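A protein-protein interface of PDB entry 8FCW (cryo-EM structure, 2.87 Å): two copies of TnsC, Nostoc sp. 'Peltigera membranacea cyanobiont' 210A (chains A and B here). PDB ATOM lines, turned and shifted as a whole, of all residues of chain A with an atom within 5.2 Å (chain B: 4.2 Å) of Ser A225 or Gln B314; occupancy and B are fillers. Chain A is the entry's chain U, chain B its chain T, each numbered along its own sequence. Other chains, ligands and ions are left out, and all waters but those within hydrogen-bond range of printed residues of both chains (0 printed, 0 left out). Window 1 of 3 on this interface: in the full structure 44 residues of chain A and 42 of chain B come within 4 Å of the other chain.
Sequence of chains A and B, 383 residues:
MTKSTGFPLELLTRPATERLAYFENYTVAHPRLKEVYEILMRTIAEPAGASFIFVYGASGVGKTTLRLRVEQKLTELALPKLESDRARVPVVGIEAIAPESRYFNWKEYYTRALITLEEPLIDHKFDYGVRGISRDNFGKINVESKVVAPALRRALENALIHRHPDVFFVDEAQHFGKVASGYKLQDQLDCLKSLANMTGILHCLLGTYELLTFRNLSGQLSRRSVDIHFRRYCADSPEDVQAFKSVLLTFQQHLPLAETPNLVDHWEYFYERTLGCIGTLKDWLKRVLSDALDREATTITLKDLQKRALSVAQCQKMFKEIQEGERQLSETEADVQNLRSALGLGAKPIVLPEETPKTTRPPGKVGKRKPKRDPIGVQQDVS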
ATOM      1  N   ALA A  50     -23.269  27.454  26.193  1.00  0.00           N
ATOM      2  CA  ALA A  50     -22.266  26.736  25.455  1.00  0.00           C
ATOM      3  C   ALA A  50     -21.171  26.219  26.336  1.00  0.00           C
ATOM      4  O   ALA A  50     -20.756  26.895  27.262  1.00  0.00           O
ATOM      5  CB  ALA A  50     -21.683  27.642  24.391  1.00  0.00           C
ATOM      6  N   SER A  51     -20.695  25.015  26.052  1.00  0.00           N
ATOM      7  CA  SER A  51     -19.632  24.401  26.823  1.00  0.00           C
ATOM      8  C   SER A  51     -18.350  24.145  26.050  1.00  0.00           C
ATOM      9  O   SER A  51     -17.319  23.784  26.648  1.00  0.00           O
ATOM     10  CB  SER A  51     -20.091  23.088  27.426  1.00  0.00           C
ATOM     11  OG  SER A  51     -20.847  22.329  26.512  1.00  0.00           O
ATOM     12  N   PHE A  52     -18.371  24.367  24.747  1.00  0.00           N
ATOM     13  CA  PHE A  52     -17.235  24.091  23.897  1.00  0.00           C
ATOM     14  C   PHE A  52     -17.018  25.229  22.939  1.00  0.00           C
ATOM     15  O   PHE A  52     -17.965  25.808  22.423  1.00  0.00           O
ATOM     16  CB  PHE A  52     -17.452  22.809  23.123  1.00  0.00           C
ATOM     17  CG  PHE A  52     -17.253  21.572  23.952  1.00  0.00           C
ATOM     18  CD1 PHE A  52     -16.192  21.486  24.837  1.00  0.00           C
ATOM     19  CD2 PHE A  52     -18.126  20.520  23.866  1.00  0.00           C
ATOM     20  CE1 PHE A  52     -16.017  20.380  25.620  1.00  0.00           C
ATOM     21  CE2 PHE A  52     -17.974  19.439  24.667  1.00  0.00           C
ATOM     22  CZ  PHE A  52     -16.911  19.359  25.547  1.00  0.00           C
ATOM     23  N   ILE A  53     -15.756  25.555  22.707  1.00  0.00           N
ATOM     24  CA  ILE A  53     -15.326  26.372  21.598  1.00  0.00           C
ATOM     25  C   ILE A  53     -14.304  25.570  20.820  1.00  0.00           C
ATOM     26  O   ILE A  53     -13.253  25.197  21.326  1.00  0.00           O
ATOM     27  CB  ILE A  53     -14.732  27.688  22.063  1.00  0.00           C
ATOM     28  CG1 ILE A  53     -15.678  28.426  23.004  1.00  0.00           C
ATOM     29  CG2 ILE A  53     -14.396  28.558  20.856  1.00  0.00           C
ATOM     30  CD1 ILE A  53     -15.132  28.421  24.406  1.00  0.00           C
ATOM     31  N   PHE A  54     -14.621  25.253  19.581  1.00  0.00           N
ATOM     32  CA  PHE A  54     -13.755  24.528  18.704  1.00  0.00           C
ATOM     33  C   PHE A  54     -13.054  25.532  17.799  1.00  0.00           C
ATOM     34  O   PHE A  54     -13.572  25.921  16.758  1.00  0.00           O
ATOM     35  CB  PHE A  54     -14.554  23.517  17.905  1.00  0.00           C
ATOM     36  CG  PHE A  54     -15.028  22.340  18.696  1.00  0.00           C
ATOM     37  CD1 PHE A  54     -16.256  22.376  19.317  1.00  0.00           C
ATOM     38  CD2 PHE A  54     -14.267  21.194  18.784  1.00  0.00           C
ATOM     39  CE1 PHE A  54     -16.704  21.295  20.043  1.00  0.00           C
ATOM     40  CE2 PHE A  54     -14.707  20.115  19.504  1.00  0.00           C
ATOM     41  CZ  PHE A  54     -15.915  20.169  20.137  1.00  0.00           C
ATOM     42  N   ARG A 215     -16.285  17.729  15.099  1.00  0.00           N
ATOM     43  CA  ARG A 215     -16.887  19.039  14.821  1.00  0.00           C
ATOM     44  C   ARG A 215     -18.382  18.983  15.026  1.00  0.00           C
ATOM     45  O   ARG A 215     -18.979  19.941  15.542  1.00  0.00           O
ATOM     46  CB  ARG A 215     -16.532  19.560  13.426  1.00  0.00           C
ATOM     47  CG  ARG A 215     -17.360  18.990  12.295  1.00  0.00           C
ATOM     48  CD  ARG A 215     -17.438  19.994  11.153  1.00  0.00           C
ATOM     49  NE  ARG A 215     -18.006  21.265  11.594  1.00  0.00           N
ATOM     50  CZ  ARG A 215     -18.469  22.211  10.792  1.00  0.00           C
ATOM     51  NH1 ARG A 215     -18.385  22.062   9.495  1.00  0.00           N
ATOM     52  NH2 ARG A 215     -18.985  23.316  11.297  1.00  0.00           N
ATOM     53  N   ASN A 216     -19.024  17.894  14.630  1.00  0.00           N
ATOM     54  CA  ASN A 216     -20.473  17.791  14.758  1.00  0.00           C
ATOM     55  C   ASN A 216     -20.872  16.350  14.984  1.00  0.00           C
ATOM     56  O   ASN A 216     -21.016  15.575  14.045  1.00  0.00           O
ATOM     57  CB  ASN A 216     -21.154  18.326  13.506  1.00  0.00           C
ATOM     58  CG  ASN A 216     -21.717  19.706  13.681  1.00  0.00           C
ATOM     59  OD1 ASN A 216     -21.879  20.170  14.794  1.00  0.00           O
ATOM     60  ND2 ASN A 216     -22.052  20.353  12.573  1.00  0.00           N
ATOM     61  N   LEU A 221     -24.179  18.115  21.420  1.00  0.00           N
ATOM     62  CA  LEU A 221     -22.838  18.668  21.318  1.00  0.00           C
ATOM     63  C   LEU A 221     -22.795  19.769  20.284  1.00  0.00           C
ATOM     64  O   LEU A 221     -21.987  20.679  20.380  1.00  0.00           O
ATOM     65  CB  LEU A 221     -21.833  17.578  20.988  1.00  0.00           C
ATOM     66  CG  LEU A 221     -21.501  16.610  22.108  1.00  0.00           C
ATOM     67  CD1 LEU A 221     -20.774  15.399  21.534  1.00  0.00           C
ATOM     68  CD2 LEU A 221     -20.663  17.282  23.193  1.00  0.00           C
ATOM     69  N   SER A 222     -23.643  19.699  19.274  1.00  0.00           N
ATOM     70  CA  SER A 222     -23.735  20.767  18.296  1.00  0.00           C
ATOM     71  C   SER A 222     -24.276  22.027  18.917  1.00  0.00           C
ATOM     72  O   SER A 222     -23.802  23.121  18.615  1.00  0.00           O
ATOM     73  CB  SER A 222     -24.600  20.342  17.137  1.00  0.00           C
ATOM     74  OG  SER A 222     -24.277  19.031  16.713  1.00  0.00           O
ATOM     75  N   ARG A 223     -25.262  21.904  19.785  1.00  0.00           N
ATOM     76  CA  ARG A 223     -25.867  23.062  20.419  1.00  0.00           C
ATOM     77  C   ARG A 223     -24.870  23.756  21.318  1.00  0.00           C
ATOM     78  O   ARG A 223     -24.774  24.978  21.323  1.00  0.00           O
ATOM     79  CB  ARG A 223     -27.122  22.671  21.207  1.00  0.00           C
ATOM     80  CG  ARG A 223     -28.004  23.833  21.581  1.00  0.00           C
ATOM     81  CD  ARG A 223     -29.231  23.412  22.394  1.00  0.00           C
ATOM     82  NE  ARG A 223     -28.899  23.108  23.789  1.00  0.00           N
ATOM     83  CZ  ARG A 223     -28.620  24.013  24.708  1.00  0.00           C
ATOM     84  NH1 ARG A 223     -28.627  25.288  24.416  1.00  0.00           N
ATOM     85  NH2 ARG A 223     -28.267  23.661  25.920  1.00  0.00           N
ATOM     86  N   ARG A 224     -24.116  22.987  22.089  1.00  0.00           N
ATOM     87  CA  ARG A 224     -23.255  23.529  23.111  1.00  0.00           C
ATOM     88  C   ARG A 224     -21.833  23.749  22.635  1.00  0.00           C
ATOM     89  O   ARG A 224     -20.864  23.673  23.434  1.00  0.00           O
ATOM     90  CB  ARG A 224     -23.259  22.590  24.323  1.00  0.00           C
ATOM     91  CG  ARG A 224     -24.633  22.042  24.652  1.00  0.00           C
ATOM     92  CD  ARG A 224     -24.590  21.077  25.803  1.00  0.00           C
ATOM     93  NE  ARG A 224     -24.820  21.694  27.109  1.00  0.00           N
ATOM     94  CZ  ARG A 224     -25.349  21.049  28.155  1.00  0.00           C
ATOM     95  NH1 ARG A 224     -25.700  19.779  28.062  1.00  0.00           N
ATOM     96  NH2 ARG A 224     -25.526  21.665  29.309  1.00  0.00           N
ATOM     97  N   SER A 225     -21.658  24.010  21.345  1.00  0.00           N
ATOM     98  CA  SER A 225     -20.340  24.318  20.798  1.00  0.00           C
ATOM     99  C   SER A 225     -20.457  25.438  19.803  1.00  0.00           C
ATOM    100  O   SER A 225     -21.467  25.569  19.096  1.00  0.00           O
ATOM    101  CB  SER A 225     -19.736  23.101  20.123  1.00  0.00           C
ATOM    102  OG  SER A 225     -20.437  22.755  18.948  1.00  0.00           O
ATOM    103  N   VAL A 226     -19.429  26.277  19.766  1.00  0.00           N
ATOM    104  CA  VAL A 226     -19.303  27.352  18.802  1.00  0.00           C
ATOM    105  C   VAL A 226     -18.033  27.126  17.997  1.00  0.00           C
ATOM    106  O   VAL A 226     -17.029  26.665  18.534  1.00  0.00           O
ATOM    107  CB  VAL A 226     -19.319  28.711  19.475  1.00  0.00           C
ATOM    108  CG1 VAL A 226     -20.429  28.793  20.510  1.00  0.00           C
ATOM    109  CG2 VAL A 226     -17.986  29.048  20.065  1.00  0.00           C
ATOM    110  N   ASP A 227     -18.109  27.358  16.695  1.00  0.00           N
ATOM    111  CA  ASP A 227     -17.022  27.054  15.787  1.00  0.00           C
ATOM    112  C   ASP A 227     -16.339  28.335  15.368  1.00  0.00           C
ATOM    113  O   ASP A 227     -16.936  29.172  14.698  1.00  0.00           O
ATOM    114  CB  ASP A 227     -17.566  26.321  14.565  1.00  0.00           C
ATOM    115  CG  ASP A 227     -18.011  24.910  14.869  1.00  0.00           C
ATOM    116  OD1 ASP A 227     -18.196  24.610  16.052  1.00  0.00           O
ATOM    117  OD2 ASP A 227     -18.171  24.108  13.928  1.00  0.00           O
ATOM    118  N   SER B 311     -24.237  27.744  13.115  1.00  0.00           N
ATOM    119  CA  SER B 311     -23.812  27.387  11.790  1.00  0.00           C
ATOM    120  C   SER B 311     -24.819  26.487  11.109  1.00  0.00           C
ATOM    121  O   SER B 311     -25.537  25.754  11.776  1.00  0.00           O
ATOM    122  CB  SER B 311     -22.460  26.704  11.866  1.00  0.00           C
ATOM    123  OG  SER B 311     -21.511  27.473  12.585  1.00  0.00           O
ATOM    124  N   VAL B 312     -24.905  26.555   9.784  1.00  0.00           N
ATOM    125  CA  VAL B 312     -25.838  25.715   9.049  1.00  0.00           C
ATOM    126  C   VAL B 312     -25.520  24.244   9.283  1.00  0.00           C
ATOM    127  O   VAL B 312     -26.400  23.415   9.409  1.00  0.00           O
ATOM    128  CB  VAL B 312     -25.811  26.060   7.557  1.00  0.00           C
ATOM    129  CG1 VAL B 312     -26.756  25.201   6.725  1.00  0.00           C
ATOM    130  CG2 VAL B 312     -26.125  27.527   7.347  1.00  0.00           C
ATOM    131  N   ALA B 313     -24.257  23.912   9.390  1.00  0.00           N
ATOM    132  CA  ALA B 313     -23.842  22.541   9.677  1.00  0.00           C
ATOM    133  C   ALA B 313     -24.301  22.118  11.043  1.00  0.00           C
ATOM    134  O   ALA B 313     -24.690  20.971  11.249  1.00  0.00           O
ATOM    135  CB  ALA B 313     -22.338  22.419   9.576  1.00  0.00           C
ATOM    136  N   GLN B 314     -24.262  23.029  12.005  1.00  0.00           N
ATOM    137  CA  GLN B 314     -24.694  22.720  13.358  1.00  0.00           C
ATOM    138  C   GLN B 314     -26.168  22.427  13.353  1.00  0.00           C
ATOM    139  O   GLN B 314     -26.616  21.421  13.918  1.00  0.00           O
ATOM    140  CB  GLN B 314     -24.355  23.845  14.326  1.00  0.00           C
ATOM    141  CG  GLN B 314     -22.879  24.126  14.466  1.00  0.00           C
ATOM    142  CD  GLN B 314     -22.571  25.163  15.524  1.00  0.00           C
ATOM    143  OE1 GLN B 314     -22.047  26.248  15.220  1.00  0.00           O
ATOM    144  NE2 GLN B 314     -22.861  24.825  16.775  1.00  0.00           N
ATOM    145  N   CYS B 315     -26.950  23.284  12.715  1.00  0.00           N
ATOM    146  CA  CYS B 315     -28.386  23.140  12.715  1.00  0.00           C
ATOM    147  C   CYS B 315     -28.805  21.956  11.872  1.00  0.00           C
ATOM    148  O   CYS B 315     -29.815  21.333  12.153  1.00  0.00           O
ATOM    149  CB  CYS B 315     -29.043  24.404  12.206  1.00  0.00           C
ATOM    150  SG  CYS B 315     -28.947  25.788  13.324  1.00  0.00           S
ATOM    151  N   GLN B 316     -28.056  21.636  10.838  1.00  0.00           N
ATOM    152  CA  GLN B 316     -28.423  20.525   9.975  1.00  0.00           C
ATOM    153  C   GLN B 316     -28.293  19.229  10.717  1.00  0.00           C
ATOM    154  O   GLN B 316     -29.093  18.327  10.530  1.00  0.00           O
ATOM    155  CB  GLN B 316     -27.566  20.513   8.716  1.00  0.00           C
ATOM    156  CG  GLN B 316     -28.273  19.969   7.493  1.00  0.00           C
ATOM    157  CD  GLN B 316     -27.795  20.627   6.214  1.00  0.00           C
ATOM    158  OE1 GLN B 316     -26.739  21.241   6.194  1.00  0.00           O
ATOM    159  NE2 GLN B 316     -28.577  20.505   5.145  1.00  0.00           N
ATOM    160  N   LYS B 317     -27.314  19.121  11.590  1.00  0.00           N
ATOM    161  CA  LYS B 317     -27.170  17.927  12.409  1.00  0.00           C
ATOM    162  C   LYS B 317     -28.269  17.874  13.440  1.00  0.00           C
ATOM    163  O   LYS B 317     -28.768  16.807  13.773  1.00  0.00           O
ATOM    164  CB  LYS B 317     -25.802  17.864  13.063  1.00  0.00           C
ATOM    165  CG  LYS B 317     -25.719  17.013  14.320  1.00  0.00           C
ATOM    166  CD  LYS B 317     -25.803  15.529  14.007  1.00  0.00           C
ATOM    167  CE  LYS B 317     -24.465  14.874  14.070  1.00  0.00           C
ATOM    168  NZ  LYS B 317     -24.482  13.420  13.796  1.00  0.00           N
ATOM    169  N   MET B 318     -28.680  19.016  13.954  1.00  0.00           N
ATOM    170  CA  MET B 318     -29.799  19.076  14.873  1.00  0.00           C
ATOM    171  C   MET B 318     -31.047  18.483  14.257  1.00  0.00           C
ATOM    172  O   MET B 318     -31.705  17.656  14.865  1.00  0.00           O
ATOM    173  CB  MET B 318     -30.082  20.511  15.265  1.00  0.00           C
ATOM    174  CG  MET B 318     -28.957  21.281  15.909  1.00  0.00           C
ATOM    175  SD  MET B 318     -29.697  22.318  17.170  1.00  0.00           S
ATOM    176  CE  MET B 318     -28.241  22.980  17.905  1.00  0.00           C
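OG of Ser B311 is in hydrogen-bond range of OE1 of Gln B314 (3.0 Å).
NH2 of Arg A215 lies within salt-bridge range of OD2 of Asp A227, at 2.9 Å.
The side-chain hydroxyl (OG) of Ser A222 lies within hydrogen-bond range of the side-chain amide oxygen (OD1) of Asn A216 (3.3 Å).
The backbone carbonyl oxygen (O) of Leu A221 lies within hydrogen-bond range of the side-chain hydroxyl (OG) of Ser A225 (3.0 Å).
The side-chain hydroxyl (OG) of Ser A225 sits at hydrogen-bond distance from the backbone carbonyl oxygen (O) of Ser A222 (3.4 Å).
The backbone carbonyl oxygen of Ala B313 lies within hydrogen-bond range of the side-chain amide nitrogen of Asn A216.
The side-chain amide nitrogen (NE2) of Gln B314 is in hydrogen-bond range of the backbone carbonyl oxygen (O) of Ser A222, 2.7 Å away.
O of Ser A225 is in hydrogen-bond range of NE2 of Gln B314.
Of the printed residues of chain B, Arg A215 touches Ala B313 (3.9 Å).
Of the printed residues of chain B, Asn A216 touches Ala B313, Gln B314 and Lys B317.
Printed residues of chain B within 4 Å of Ser A222: Gln B314 (2.7 Å) and Lys B317 (3.4 Å).
Of the printed residues of chain B, Arg A223 touches Met B318 (3.5 Å).
Ser A225 touches just one residue of chain B: Gln B314.
Of chain A, only Asn A216 (3.5 Å), Ser A222 (2.7 Å) and Ser A225 (2.8 Å) come within 4 Å of Gln B314.
Of the printed residues of chain A, Lys B317 touches Asn A216 and Ser A222.
The nearest printed residue of chain B that does not touch Ser A225 is Ser B311 (6.8 Å).
The nearest residue of chain A that does not touch Gln B314 is Asp A227 (4.3 Å).
The nearest printed residue of chain B that does not touch Arg A215 is Ser B311 (4.9 Å).
Of the 14 printed residues of chain A, 5 touch a printed residue of chain B.
Of the 8 printed residues of chain B, 4 touch a printed residue of chain A.
Among the printed residues, 8 pairs touch across the chains.
Among the printed residues, no Asp or Glu carboxylate lies within 4 Å of a Lys or Arg side-chain nitrogen of the other chain.
No position is printed for both chains.
Of the 8 pairs that touch across the chains among the printed residues, none has its exchanged pair printed and touching as well.
Among the printed residues, merely in contact across the chains: Arg A215 with Ala B313 (3.9 Å), Asn A216 with Gln B314 (3.5 Å), Asn A216 with Lys B317 (3.5 Å), Ser A222 with Lys B317 (3.4 Å) and Arg A223 with Met B318 (3.5 Å).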
